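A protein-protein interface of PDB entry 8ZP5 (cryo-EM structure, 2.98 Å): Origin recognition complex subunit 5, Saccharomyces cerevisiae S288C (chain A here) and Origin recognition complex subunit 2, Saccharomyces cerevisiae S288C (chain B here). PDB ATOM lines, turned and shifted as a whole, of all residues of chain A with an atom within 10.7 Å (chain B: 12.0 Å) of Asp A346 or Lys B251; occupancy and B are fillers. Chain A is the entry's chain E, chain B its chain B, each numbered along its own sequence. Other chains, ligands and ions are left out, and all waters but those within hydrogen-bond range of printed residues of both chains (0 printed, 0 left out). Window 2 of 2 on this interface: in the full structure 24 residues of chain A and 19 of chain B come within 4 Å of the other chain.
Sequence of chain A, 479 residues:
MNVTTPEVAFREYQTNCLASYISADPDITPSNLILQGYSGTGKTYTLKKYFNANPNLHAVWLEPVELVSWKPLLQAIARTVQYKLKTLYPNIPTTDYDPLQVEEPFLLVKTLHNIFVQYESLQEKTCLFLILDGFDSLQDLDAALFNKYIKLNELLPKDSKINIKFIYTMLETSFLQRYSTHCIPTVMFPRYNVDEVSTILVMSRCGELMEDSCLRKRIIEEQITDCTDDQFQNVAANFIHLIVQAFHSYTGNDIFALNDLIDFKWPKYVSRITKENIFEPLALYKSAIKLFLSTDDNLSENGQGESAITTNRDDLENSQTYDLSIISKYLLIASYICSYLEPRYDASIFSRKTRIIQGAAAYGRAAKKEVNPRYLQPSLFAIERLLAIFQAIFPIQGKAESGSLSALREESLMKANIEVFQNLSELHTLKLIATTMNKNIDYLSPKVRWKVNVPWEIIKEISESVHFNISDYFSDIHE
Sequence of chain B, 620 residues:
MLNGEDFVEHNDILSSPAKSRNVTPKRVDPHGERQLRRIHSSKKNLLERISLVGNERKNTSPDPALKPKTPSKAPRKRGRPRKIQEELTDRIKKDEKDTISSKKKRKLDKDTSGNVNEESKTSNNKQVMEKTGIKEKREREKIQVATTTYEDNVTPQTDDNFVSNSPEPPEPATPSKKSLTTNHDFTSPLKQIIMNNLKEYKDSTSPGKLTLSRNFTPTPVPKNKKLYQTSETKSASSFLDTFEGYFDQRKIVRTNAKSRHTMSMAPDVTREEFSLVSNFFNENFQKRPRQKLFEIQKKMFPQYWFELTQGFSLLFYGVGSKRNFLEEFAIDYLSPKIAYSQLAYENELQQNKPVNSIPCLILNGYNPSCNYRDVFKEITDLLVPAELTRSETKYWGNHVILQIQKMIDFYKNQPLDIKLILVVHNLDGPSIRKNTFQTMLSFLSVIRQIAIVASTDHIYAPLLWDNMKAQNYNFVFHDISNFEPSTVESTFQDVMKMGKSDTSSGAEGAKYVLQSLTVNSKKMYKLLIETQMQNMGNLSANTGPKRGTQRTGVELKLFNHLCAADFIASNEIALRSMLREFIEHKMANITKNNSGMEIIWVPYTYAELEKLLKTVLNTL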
ATOM      1  N   LEU A 341       0.066 -29.370  31.388  1.00  0.00           N
ATOM      2  CA  LEU A 341       1.500 -29.521  31.173  1.00  0.00           C
ATOM      3  C   LEU A 341       2.004 -28.297  30.423  1.00  0.00           C
ATOM      4  O   LEU A 341       1.373 -27.850  29.461  1.00  0.00           O
ATOM      5  CB  LEU A 341       1.806 -30.818  30.410  1.00  0.00           C
ATOM      6  CG  LEU A 341       3.246 -31.316  30.260  1.00  0.00           C
ATOM      7  CD1 LEU A 341       3.243 -32.827  30.098  1.00  0.00           C
ATOM      8  CD2 LEU A 341       3.962 -30.677  29.090  1.00  0.00           C
ATOM      9  N   GLU A 342       3.139 -27.760  30.868  1.00  0.00           N
ATOM     10  CA  GLU A 342       3.627 -26.487  30.360  1.00  0.00           C
ATOM     11  C   GLU A 342       4.042 -26.603  28.893  1.00  0.00           C
ATOM     12  O   GLU A 342       4.429 -27.678  28.431  1.00  0.00           O
ATOM     13  CB  GLU A 342       4.810 -26.003  31.192  1.00  0.00           C
ATOM     14  CG  GLU A 342       4.451 -25.635  32.622  1.00  0.00           C
ATOM     15  CD  GLU A 342       5.646 -25.142  33.413  1.00  0.00           C
ATOM     16  OE1 GLU A 342       6.775 -25.198  32.883  1.00  0.00           O
ATOM     17  OE2 GLU A 342       5.456 -24.698  34.564  1.00  0.00           O
ATOM     18  N   PRO A 343       3.979 -25.500  28.137  1.00  0.00           N
ATOM     19  CA  PRO A 343       4.374 -25.557  26.722  1.00  0.00           C
ATOM     20  C   PRO A 343       5.870 -25.747  26.531  1.00  0.00           C
ATOM     21  O   PRO A 343       6.553 -24.873  25.986  1.00  0.00           O
ATOM     22  CB  PRO A 343       3.910 -24.199  26.172  1.00  0.00           C
ATOM     23  CG  PRO A 343       2.908 -23.696  27.163  1.00  0.00           C
ATOM     24  CD  PRO A 343       3.370 -24.207  28.486  1.00  0.00           C
ATOM     25  N   ARG A 344       6.387 -26.891  26.976  1.00  0.00           N
ATOM     26  CA  ARG A 344       7.774 -27.282  26.761  1.00  0.00           C
ATOM     27  C   ARG A 344       7.852 -28.526  25.883  1.00  0.00           C
ATOM     28  O   ARG A 344       8.785 -29.324  25.995  1.00  0.00           O
ATOM     29  CB  ARG A 344       8.490 -27.512  28.091  1.00  0.00           C
ATOM     30  CG  ARG A 344       7.879 -28.605  28.953  1.00  0.00           C
ATOM     31  CD  ARG A 344       8.670 -28.803  30.235  1.00  0.00           C
ATOM     32  NE  ARG A 344       8.661 -27.612  31.075  1.00  0.00           N
ATOM     33  CZ  ARG A 344       9.700 -26.807  31.245  1.00  0.00           C
ATOM     34  NH1 ARG A 344      10.857 -27.035  30.644  1.00  0.00           N
ATOM     35  NH2 ARG A 344       9.578 -25.746  32.039  1.00  0.00           N
ATOM     36  N   TYR A 345       6.865 -28.691  25.000  1.00  0.00           N
ATOM     37  CA  TYR A 345       6.783 -29.872  24.151  1.00  0.00           C
ATOM     38  C   TYR A 345       7.871 -29.891  23.089  1.00  0.00           C
ATOM     39  O   TYR A 345       8.075 -30.923  22.441  1.00  0.00           O
ATOM     40  CB  TYR A 345       5.415 -29.920  23.475  1.00  0.00           C
ATOM     41  CG  TYR A 345       4.274 -30.133  24.434  1.00  0.00           C
ATOM     42  CD1 TYR A 345       3.961 -31.396  24.909  1.00  0.00           C
ATOM     43  CD2 TYR A 345       3.508 -29.060  24.870  1.00  0.00           C
ATOM     44  CE1 TYR A 345       2.914 -31.587  25.791  1.00  0.00           C
ATOM     45  CE2 TYR A 345       2.463 -29.239  25.748  1.00  0.00           C
ATOM     46  CZ  TYR A 345       2.168 -30.503  26.205  1.00  0.00           C
ATOM     47  OH  TYR A 345       1.124 -30.676  27.084  1.00  0.00           O
ATOM     48  N   ASP A 346       8.567 -28.771  22.898  1.00  0.00           N
ATOM     49  CA  ASP A 346       9.501 -28.631  21.790  1.00  0.00           C
ATOM     50  C   ASP A 346      10.807 -29.376  22.027  1.00  0.00           C
ATOM     51  O   ASP A 346      11.526 -29.658  21.063  1.00  0.00           O
ATOM     52  CB  ASP A 346       9.794 -27.151  21.557  1.00  0.00           C
ATOM     53  CG  ASP A 346       8.555 -26.366  21.186  1.00  0.00           C
ATOM     54  OD1 ASP A 346       7.625 -26.960  20.605  1.00  0.00           O
ATOM     55  OD2 ASP A 346       8.507 -25.156  21.488  1.00  0.00           O
ATOM     56  N   ALA A 347      11.130 -29.701  23.279  1.00  0.00           N
ATOM     57  CA  ALA A 347      12.471 -30.185  23.592  1.00  0.00           C
ATOM     58  C   ALA A 347      12.632 -31.668  23.272  1.00  0.00           C
ATOM     59  O   ALA A 347      13.412 -32.040  22.389  1.00  0.00           O
ATOM     60  CB  ALA A 347      12.791 -29.915  25.065  1.00  0.00           C
ATOM     61  N   SER A 348      11.903 -32.531  23.980  1.00  0.00           N
ATOM     62  CA  SER A 348      12.115 -33.970  23.872  1.00  0.00           C
ATOM     63  C   SER A 348      10.904 -34.706  23.311  1.00  0.00           C
ATOM     64  O   SER A 348      11.038 -35.428  22.318  1.00  0.00           O
ATOM     65  CB  SER A 348      12.501 -34.540  25.244  1.00  0.00           C
ATOM     66  OG  SER A 348      13.550 -33.787  25.829  1.00  0.00           O
ATOM     67  N   ILE A 349       9.727 -34.547  23.913  1.00  0.00           N
ATOM     68  CA  ILE A 349       8.573 -35.373  23.571  1.00  0.00           C
ATOM     69  C   ILE A 349       7.898 -34.858  22.308  1.00  0.00           C
ATOM     70  O   ILE A 349       8.119 -33.715  21.891  1.00  0.00           O
ATOM     71  CB  ILE A 349       7.582 -35.441  24.748  1.00  0.00           C
ATOM     72  CG1 ILE A 349       7.043 -34.050  25.078  1.00  0.00           C
ATOM     73  CG2 ILE A 349       8.245 -36.063  25.965  1.00  0.00           C
ATOM     74  CD1 ILE A 349       5.899 -34.070  26.064  1.00  0.00           C
ATOM     75  N   PHE A 350       7.071 -35.707  21.691  1.00  0.00           N
ATOM     76  CA  PHE A 350       6.434 -35.423  20.403  1.00  0.00           C
ATOM     77  C   PHE A 350       7.455 -35.079  19.323  1.00  0.00           C
ATOM     78  O   PHE A 350       7.209 -34.212  18.479  1.00  0.00           O
ATOM     79  CB  PHE A 350       5.383 -34.314  20.525  1.00  0.00           C
ATOM     80  CG  PHE A 350       4.309 -34.603  21.532  1.00  0.00           C
ATOM     81  CD1 PHE A 350       3.944 -35.908  21.819  1.00  0.00           C
ATOM     82  CD2 PHE A 350       3.653 -33.574  22.184  1.00  0.00           C
ATOM     83  CE1 PHE A 350       2.952 -36.179  22.737  1.00  0.00           C
ATOM     84  CE2 PHE A 350       2.658 -33.842  23.104  1.00  0.00           C
ATOM     85  CZ  PHE A 350       2.310 -35.145  23.382  1.00  0.00           C
ATOM     86  N   SER A 351       8.597 -35.762  19.346  1.00  0.00           N
ATOM     87  CA  SER A 351       9.629 -35.638  18.317  1.00  0.00           C
ATOM     88  C   SER A 351      10.048 -34.190  18.068  1.00  0.00           C
ATOM     89  O   SER A 351       9.934 -33.339  18.950  1.00  0.00           O
ATOM     90  CB  SER A 351       9.148 -36.274  17.010  1.00  0.00           C
ATOM     91  OG  SER A 351      10.210 -36.399  16.081  1.00  0.00           O
ATOM     92  N   ARG A 385      -2.833 -25.450  19.365  1.00  0.00           N
ATOM     93  CA  ARG A 385      -2.030 -26.317  20.222  1.00  0.00           C
ATOM     94  C   ARG A 385      -2.761 -27.617  20.531  1.00  0.00           C
ATOM     95  O   ARG A 385      -2.152 -28.695  20.529  1.00  0.00           O
ATOM     96  CB  ARG A 385      -1.662 -25.585  21.511  1.00  0.00           C
ATOM     97  CG  ARG A 385      -0.713 -26.358  22.405  1.00  0.00           C
ATOM     98  CD  ARG A 385       0.098 -25.428  23.290  1.00  0.00           C
ATOM     99  NE  ARG A 385       0.669 -26.127  24.436  1.00  0.00           N
ATOM    100  CZ  ARG A 385       0.262 -25.966  25.687  1.00  0.00           C
ATOM    101  NH1 ARG A 385      -0.717 -25.131  25.994  1.00  0.00           N
ATOM    102  NH2 ARG A 385       0.849 -26.663  26.656  1.00  0.00           N
ATOM    103  N   ALA A 388      -2.557 -29.773  17.428  1.00  0.00           N
ATOM    104  CA  ALA A 388      -1.219 -30.325  17.256  1.00  0.00           C
ATOM    105  C   ALA A 388      -0.966 -31.476  18.222  1.00  0.00           C
ATOM    106  O   ALA A 388      -0.414 -32.511  17.833  1.00  0.00           O
ATOM    107  CB  ALA A 388      -0.172 -29.231  17.442  1.00  0.00           C
ATOM    108  N   ILE A 389      -1.374 -31.321  19.483  1.00  0.00           N
ATOM    109  CA  ILE A 389      -1.185 -32.400  20.449  1.00  0.00           C
ATOM    110  C   ILE A 389      -2.059 -33.597  20.093  1.00  0.00           C
ATOM    111  O   ILE A 389      -1.643 -34.753  20.243  1.00  0.00           O
ATOM    112  CB  ILE A 389      -1.461 -31.891  21.875  1.00  0.00           C
ATOM    113  CG1 ILE A 389      -0.430 -30.830  22.262  1.00  0.00           C
ATOM    114  CG2 ILE A 389      -1.439 -33.040  22.869  1.00  0.00           C
ATOM    115  CD1 ILE A 389      -0.376 -30.533  23.739  1.00  0.00           C
ATOM    116  N   ALA A 392      -0.340 -35.375  17.423  1.00  0.00           N
ATOM    117  CA  ALA A 392       0.849 -36.033  17.954  1.00  0.00           C
ATOM    118  C   ALA A 392       0.503 -37.337  18.663  1.00  0.00           C
ATOM    119  O   ALA A 392       1.198 -38.345  18.494  1.00  0.00           O
ATOM    120  CB  ALA A 392       1.585 -35.092  18.905  1.00  0.00           C
ATOM    121  N   TYR A 473       3.275 -39.576  30.873  1.00  0.00           N
ATOM    122  CA  TYR A 473       3.505 -38.199  30.450  1.00  0.00           C
ATOM    123  C   TYR A 473       3.543 -37.252  31.642  1.00  0.00           C
ATOM    124  O   TYR A 473       4.379 -36.342  31.694  1.00  0.00           O
ATOM    125  CB  TYR A 473       2.425 -37.763  29.462  1.00  0.00           C
ATOM    126  CG  TYR A 473       2.735 -38.112  28.028  1.00  0.00           C
ATOM    127  CD1 TYR A 473       2.736 -39.431  27.598  1.00  0.00           C
ATOM    128  CD2 TYR A 473       3.038 -37.122  27.106  1.00  0.00           C
ATOM    129  CE1 TYR A 473       3.021 -39.753  26.286  1.00  0.00           C
ATOM    130  CE2 TYR A 473       3.326 -37.435  25.797  1.00  0.00           C
ATOM    131  CZ  TYR A 473       3.316 -38.751  25.390  1.00  0.00           C
ATOM    132  OH  TYR A 473       3.603 -39.063  24.080  1.00  0.00           O
ATOM    133  N   PHE B 239      11.637 -28.773   8.480  1.00  0.00           N
ATOM    134  CA  PHE B 239      10.426 -29.574   8.337  1.00  0.00           C
ATOM    135  C   PHE B 239       9.189 -28.794   8.778  1.00  0.00           C
ATOM    136  O   PHE B 239       9.189 -28.143   9.824  1.00  0.00           O
ATOM    137  CB  PHE B 239      10.558 -30.884   9.123  1.00  0.00           C
ATOM    138  CG  PHE B 239      10.805 -30.695  10.594  1.00  0.00           C
ATOM    139  CD1 PHE B 239      12.097 -30.619  11.086  1.00  0.00           C
ATOM    140  CD2 PHE B 239       9.750 -30.623  11.488  1.00  0.00           C
ATOM    141  CE1 PHE B 239      12.333 -30.453  12.437  1.00  0.00           C
ATOM    142  CE2 PHE B 239       9.981 -30.457  12.839  1.00  0.00           C
ATOM    143  CZ  PHE B 239      11.273 -30.374  13.314  1.00  0.00           C
ATOM    144  N   LEU B 240       8.143 -28.852   7.957  1.00  0.00           N
ATOM    145  CA  LEU B 240       6.919 -28.093   8.180  1.00  0.00           C
ATOM    146  C   LEU B 240       5.728 -29.004   7.903  1.00  0.00           C
ATOM    147  O   LEU B 240       5.873 -30.222   7.752  1.00  0.00           O
ATOM    148  CB  LEU B 240       6.874 -26.840   7.293  1.00  0.00           C
ATOM    149  CG  LEU B 240       7.682 -25.584   7.630  1.00  0.00           C
ATOM    150  CD1 LEU B 240       9.170 -25.776   7.408  1.00  0.00           C
ATOM    151  CD2 LEU B 240       7.177 -24.436   6.791  1.00  0.00           C
ATOM    152  N   THR B 242       3.284 -30.149   9.596  1.00  0.00           N
ATOM    153  CA  THR B 242       3.014 -31.226  10.538  1.00  0.00           C
ATOM    154  C   THR B 242       3.050 -30.620  11.936  1.00  0.00           C
ATOM    155  O   THR B 242       3.551 -29.509  12.128  1.00  0.00           O
ATOM    156  CB  THR B 242       4.035 -32.369  10.373  1.00  0.00           C
ATOM    157  OG1 THR B 242       4.005 -32.845   9.022  1.00  0.00           O
ATOM    158  CG2 THR B 242       3.712 -33.550  11.269  1.00  0.00           C
ATOM    159  N   PHE B 243       2.487 -31.347  12.908  1.00  0.00           N
ATOM    160  CA  PHE B 243       2.568 -30.910  14.299  1.00  0.00           C
ATOM    161  C   PHE B 243       4.010 -30.670  14.727  1.00  0.00           C
ATOM    162  O   PHE B 243       4.278 -29.763  15.525  1.00  0.00           O
ATOM    163  CB  PHE B 243       1.908 -31.940  15.219  1.00  0.00           C
ATOM    164  CG  PHE B 243       2.716 -33.194  15.406  1.00  0.00           C
ATOM    165  CD1 PHE B 243       2.680 -34.203  14.461  1.00  0.00           C
ATOM    166  CD2 PHE B 243       3.519 -33.361  16.521  1.00  0.00           C
ATOM    167  CE1 PHE B 243       3.424 -35.356  14.625  1.00  0.00           C
ATOM    168  CE2 PHE B 243       4.265 -34.511  16.690  1.00  0.00           C
ATOM    169  CZ  PHE B 243       4.216 -35.510  15.741  1.00  0.00           C
ATOM    170  N   GLU B 244       4.948 -31.467  14.210  1.00  0.00           N
ATOM    171  CA  GLU B 244       6.357 -31.228  14.500  1.00  0.00           C
ATOM    172  C   GLU B 244       6.807 -29.887  13.940  1.00  0.00           C
ATOM    173  O   GLU B 244       7.639 -29.203  14.546  1.00  0.00           O
ATOM    174  CB  GLU B 244       7.211 -32.368  13.945  1.00  0.00           C
ATOM    175  CG  GLU B 244       7.023 -32.629  12.463  1.00  0.00           C
ATOM    176  CD  GLU B 244       7.658 -33.931  12.015  1.00  0.00           C
ATOM    177  OE1 GLU B 244       7.237 -34.998  12.507  1.00  0.00           O
ATOM    178  OE2 GLU B 244       8.576 -33.886  11.169  1.00  0.00           O
ATOM    179  N   GLY B 245       6.263 -29.487  12.789  1.00  0.00           N
ATOM    180  CA  GLY B 245       6.544 -28.154  12.278  1.00  0.00           C
ATOM    181  C   GLY B 245       6.019 -27.061  13.188  1.00  0.00           C
ATOM    182  O   GLY B 245       6.681 -26.041  13.398  1.00  0.00           O
ATOM    183  N   TYR B 246       4.820 -27.259  13.742  1.00  0.00           N
ATOM    184  CA  TYR B 246       4.276 -26.306  14.704  1.00  0.00           C
ATOM    185  C   TYR B 246       5.164 -26.200  15.934  1.00  0.00           C
ATOM    186  O   TYR B 246       5.415 -25.099  16.436  1.00  0.00           O
ATOM    187  CB  TYR B 246       2.860 -26.717  15.106  1.00  0.00           C
ATOM    188  CG  TYR B 246       2.356 -26.046  16.364  1.00  0.00           C
ATOM    189  CD1 TYR B 246       1.983 -24.711  16.362  1.00  0.00           C
ATOM    190  CD2 TYR B 246       2.257 -26.748  17.555  1.00  0.00           C
ATOM    191  CE1 TYR B 246       1.521 -24.097  17.509  1.00  0.00           C
ATOM    192  CE2 TYR B 246       1.797 -26.142  18.708  1.00  0.00           C
ATOM    193  CZ  TYR B 246       1.431 -24.816  18.679  1.00  0.00           C
ATOM    194  OH  TYR B 246       0.972 -24.208  19.823  1.00  0.00           O
ATOM    195  N   PHE B 247       5.645 -27.339  16.437  1.00  0.00           N
ATOM    196  CA  PHE B 247       6.531 -27.316  17.595  1.00  0.00           C
ATOM    197  C   PHE B 247       7.860 -26.645  17.265  1.00  0.00           C
ATOM    198  O   PHE B 247       8.408 -25.902  18.087  1.00  0.00           O
ATOM    199  CB  PHE B 247       6.752 -28.738  18.110  1.00  0.00           C
ATOM    200  CG  PHE B 247       5.525 -29.356  18.713  1.00  0.00           C
ATOM    201  CD1 PHE B 247       4.595 -28.571  19.373  1.00  0.00           C
ATOM    202  CD2 PHE B 247       5.298 -30.717  18.618  1.00  0.00           C
ATOM    203  CE1 PHE B 247       3.464 -29.132  19.930  1.00  0.00           C
ATOM    204  CE2 PHE B 247       4.168 -31.282  19.172  1.00  0.00           C
ATOM    205  CZ  PHE B 247       3.250 -30.489  19.829  1.00  0.00           C
ATOM    206  N   ASP B 248       8.392 -26.899  16.068  1.00  0.00           N
ATOM    207  CA  ASP B 248       9.656 -26.292  15.666  1.00  0.00           C
ATOM    208  C   ASP B 248       9.533 -24.780  15.528  1.00  0.00           C
ATOM    209  O   ASP B 248      10.440 -24.041  15.925  1.00  0.00           O
ATOM    210  CB  ASP B 248      10.136 -26.910  14.354  1.00  0.00           C
ATOM    211  CG  ASP B 248      11.519 -26.435  13.956  1.00  0.00           C
ATOM    212  OD1 ASP B 248      12.504 -26.867  14.590  1.00  0.00           O
ATOM    213  OD2 ASP B 248      11.620 -25.628  13.008  1.00  0.00           O
ATOM    214  N   GLN B 249       8.425 -24.299  14.964  1.00  0.00           N
ATOM    215  CA  GLN B 249       8.278 -22.868  14.730  1.00  0.00           C
ATOM    216  C   GLN B 249       7.836 -22.100  15.967  1.00  0.00           C
ATOM    217  O   GLN B 249       8.094 -20.895  16.052  1.00  0.00           O
ATOM    218  CB  GLN B 249       7.289 -22.620  13.589  1.00  0.00           C
ATOM    219  CG  GLN B 249       7.762 -23.145  12.245  1.00  0.00           C
ATOM    220  CD  GLN B 249       7.182 -22.371  11.083  1.00  0.00           C
ATOM    221  OE1 GLN B 249       6.070 -21.852  11.162  1.00  0.00           O
ATOM    222  NE2 GLN B 249       7.936 -22.286   9.995  1.00  0.00           N
ATOM    223  N   ARG B 250       7.187 -22.759  16.929  1.00  0.00           N
ATOM    224  CA  ARG B 250       6.730 -22.091  18.147  1.00  0.00           C
ATOM    225  C   ARG B 250       7.882 -22.078  19.150  1.00  0.00           C
ATOM    226  O   ARG B 250       7.902 -22.809  20.142  1.00  0.00           O
ATOM    227  CB  ARG B 250       5.494 -22.780  18.712  1.00  0.00           C
ATOM    228  CG  ARG B 250       4.596 -21.873  19.546  1.00  0.00           C
ATOM    229  CD  ARG B 250       4.998 -21.866  21.014  1.00  0.00           C
ATOM    230  NE  ARG B 250       4.983 -23.200  21.600  1.00  0.00           N
ATOM    231  CZ  ARG B 250       3.968 -23.706  22.287  1.00  0.00           C
ATOM    232  NH1 ARG B 250       2.866 -23.007  22.509  1.00  0.00           N
ATOM    233  NH2 ARG B 250       4.062 -24.942  22.768  1.00  0.00           N
ATOM    234  N   LYS B 251       8.862 -21.223  18.876  1.00  0.00           N
ATOM    235  CA  LYS B 251      10.026 -21.089  19.748  1.00  0.00           C
ATOM    236  C   LYS B 251      10.368 -19.622  19.980  1.00  0.00           C
ATOM    237  O   LYS B 251       9.656 -18.729  19.520  1.00  0.00           O
ATOM    238  CB  LYS B 251      11.233 -21.823  19.155  1.00  0.00           C
ATOM    239  CG  LYS B 251      11.041 -23.325  19.007  1.00  0.00           C
ATOM    240  CD  LYS B 251      12.331 -24.013  18.593  1.00  0.00           C
ATOM    241  CE  LYS B 251      13.184 -24.362  19.801  1.00  0.00           C
ATOM    242  NZ  LYS B 251      12.523 -25.375  20.669  1.00  0.00           N
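The side-chain carboxylate (OD1) of Asp A346 lies close to the backbone carbonyl oxygen (O) of Phe B247. The backbone carbonyl oxygen of Arg B250 sits close to the side-chain carboxylate of Asp A346 (2.8 Å).
Of chain B, only Phe B247, Arg B250 and Lys B251 come within 4 Å of Asp A346. Lys B251 touches just one residue of chain A: Asp A346 (3.4 Å). No residue of chain B comes within 4 Å of Ser A348. No residue of chain B comes within 4 Å of Ile A349. Phe B247 touches just these residues of chain A: Asp A346 (2.8 Å) and Phe A350 (3.5 Å). No residue of chain A comes within 4 Å of Asp B248. Of chain A, only Pro A343, Asp A346 and Arg A385 come within 4 Å of Arg B250. Printed residues of chain B within 4 Å of Ala A388: Phe B243 (3.5 Å) and Tyr B246 (3.5 Å). Printed residues of chain B within 4 Å of Arg A385: Tyr B246 and Arg B250. Of the printed residues of chain B, Ala A392 touches Phe B243 (3.5 Å). Printed residues of chain B within 4 Å of Phe A350: Phe B243 (3.5 Å) and Phe B247 (3.5 Å). Arg A344 touches none of the printed residues of chain B. Tyr A345 touches none of the printed residues of chain B.
Pro A343 touches Arg B250 (CB to NH2, 3.5 Å). CB of Asp A346 touches NZ of Lys B251 (3.4 Å). Phe A350 touches Phe B243. Phe A350 touches Phe B247. Arg A385 touches Tyr B246 (CB to OH, 3.4 Å). Arg A385 touches Arg B250 (CD to NH1, 3.8 Å). Ala A388 touches Phe B243. Ala A388 touches Tyr B246 (CB to CD2, 3.5 Å). Ala A392 touches Phe B243 (CB to CD2, 3.5 Å).
NH1 of Arg B250 is in hydrogen-bond range of OH of Tyr B246. The backbone carbonyl oxygen (O) of Leu A341 sits at hydrogen-bond distance from the guanidinium group (NH2) of Arg A385 (3.1 Å).
Hydrophobic or aromatic side chains of chain B within 4 Å of the printed part of chain A: Phe B243, Tyr B246 and Phe B247. Of the 16 printed residues of chain A, 6 touch a printed residue of chain B. Among the printed residues, 11 pairs touch across the chains. Among the printed residues, no Asp or Glu carboxylate lies within 4 Å of a Lys or Arg side-chain nitrogen of the other chain.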
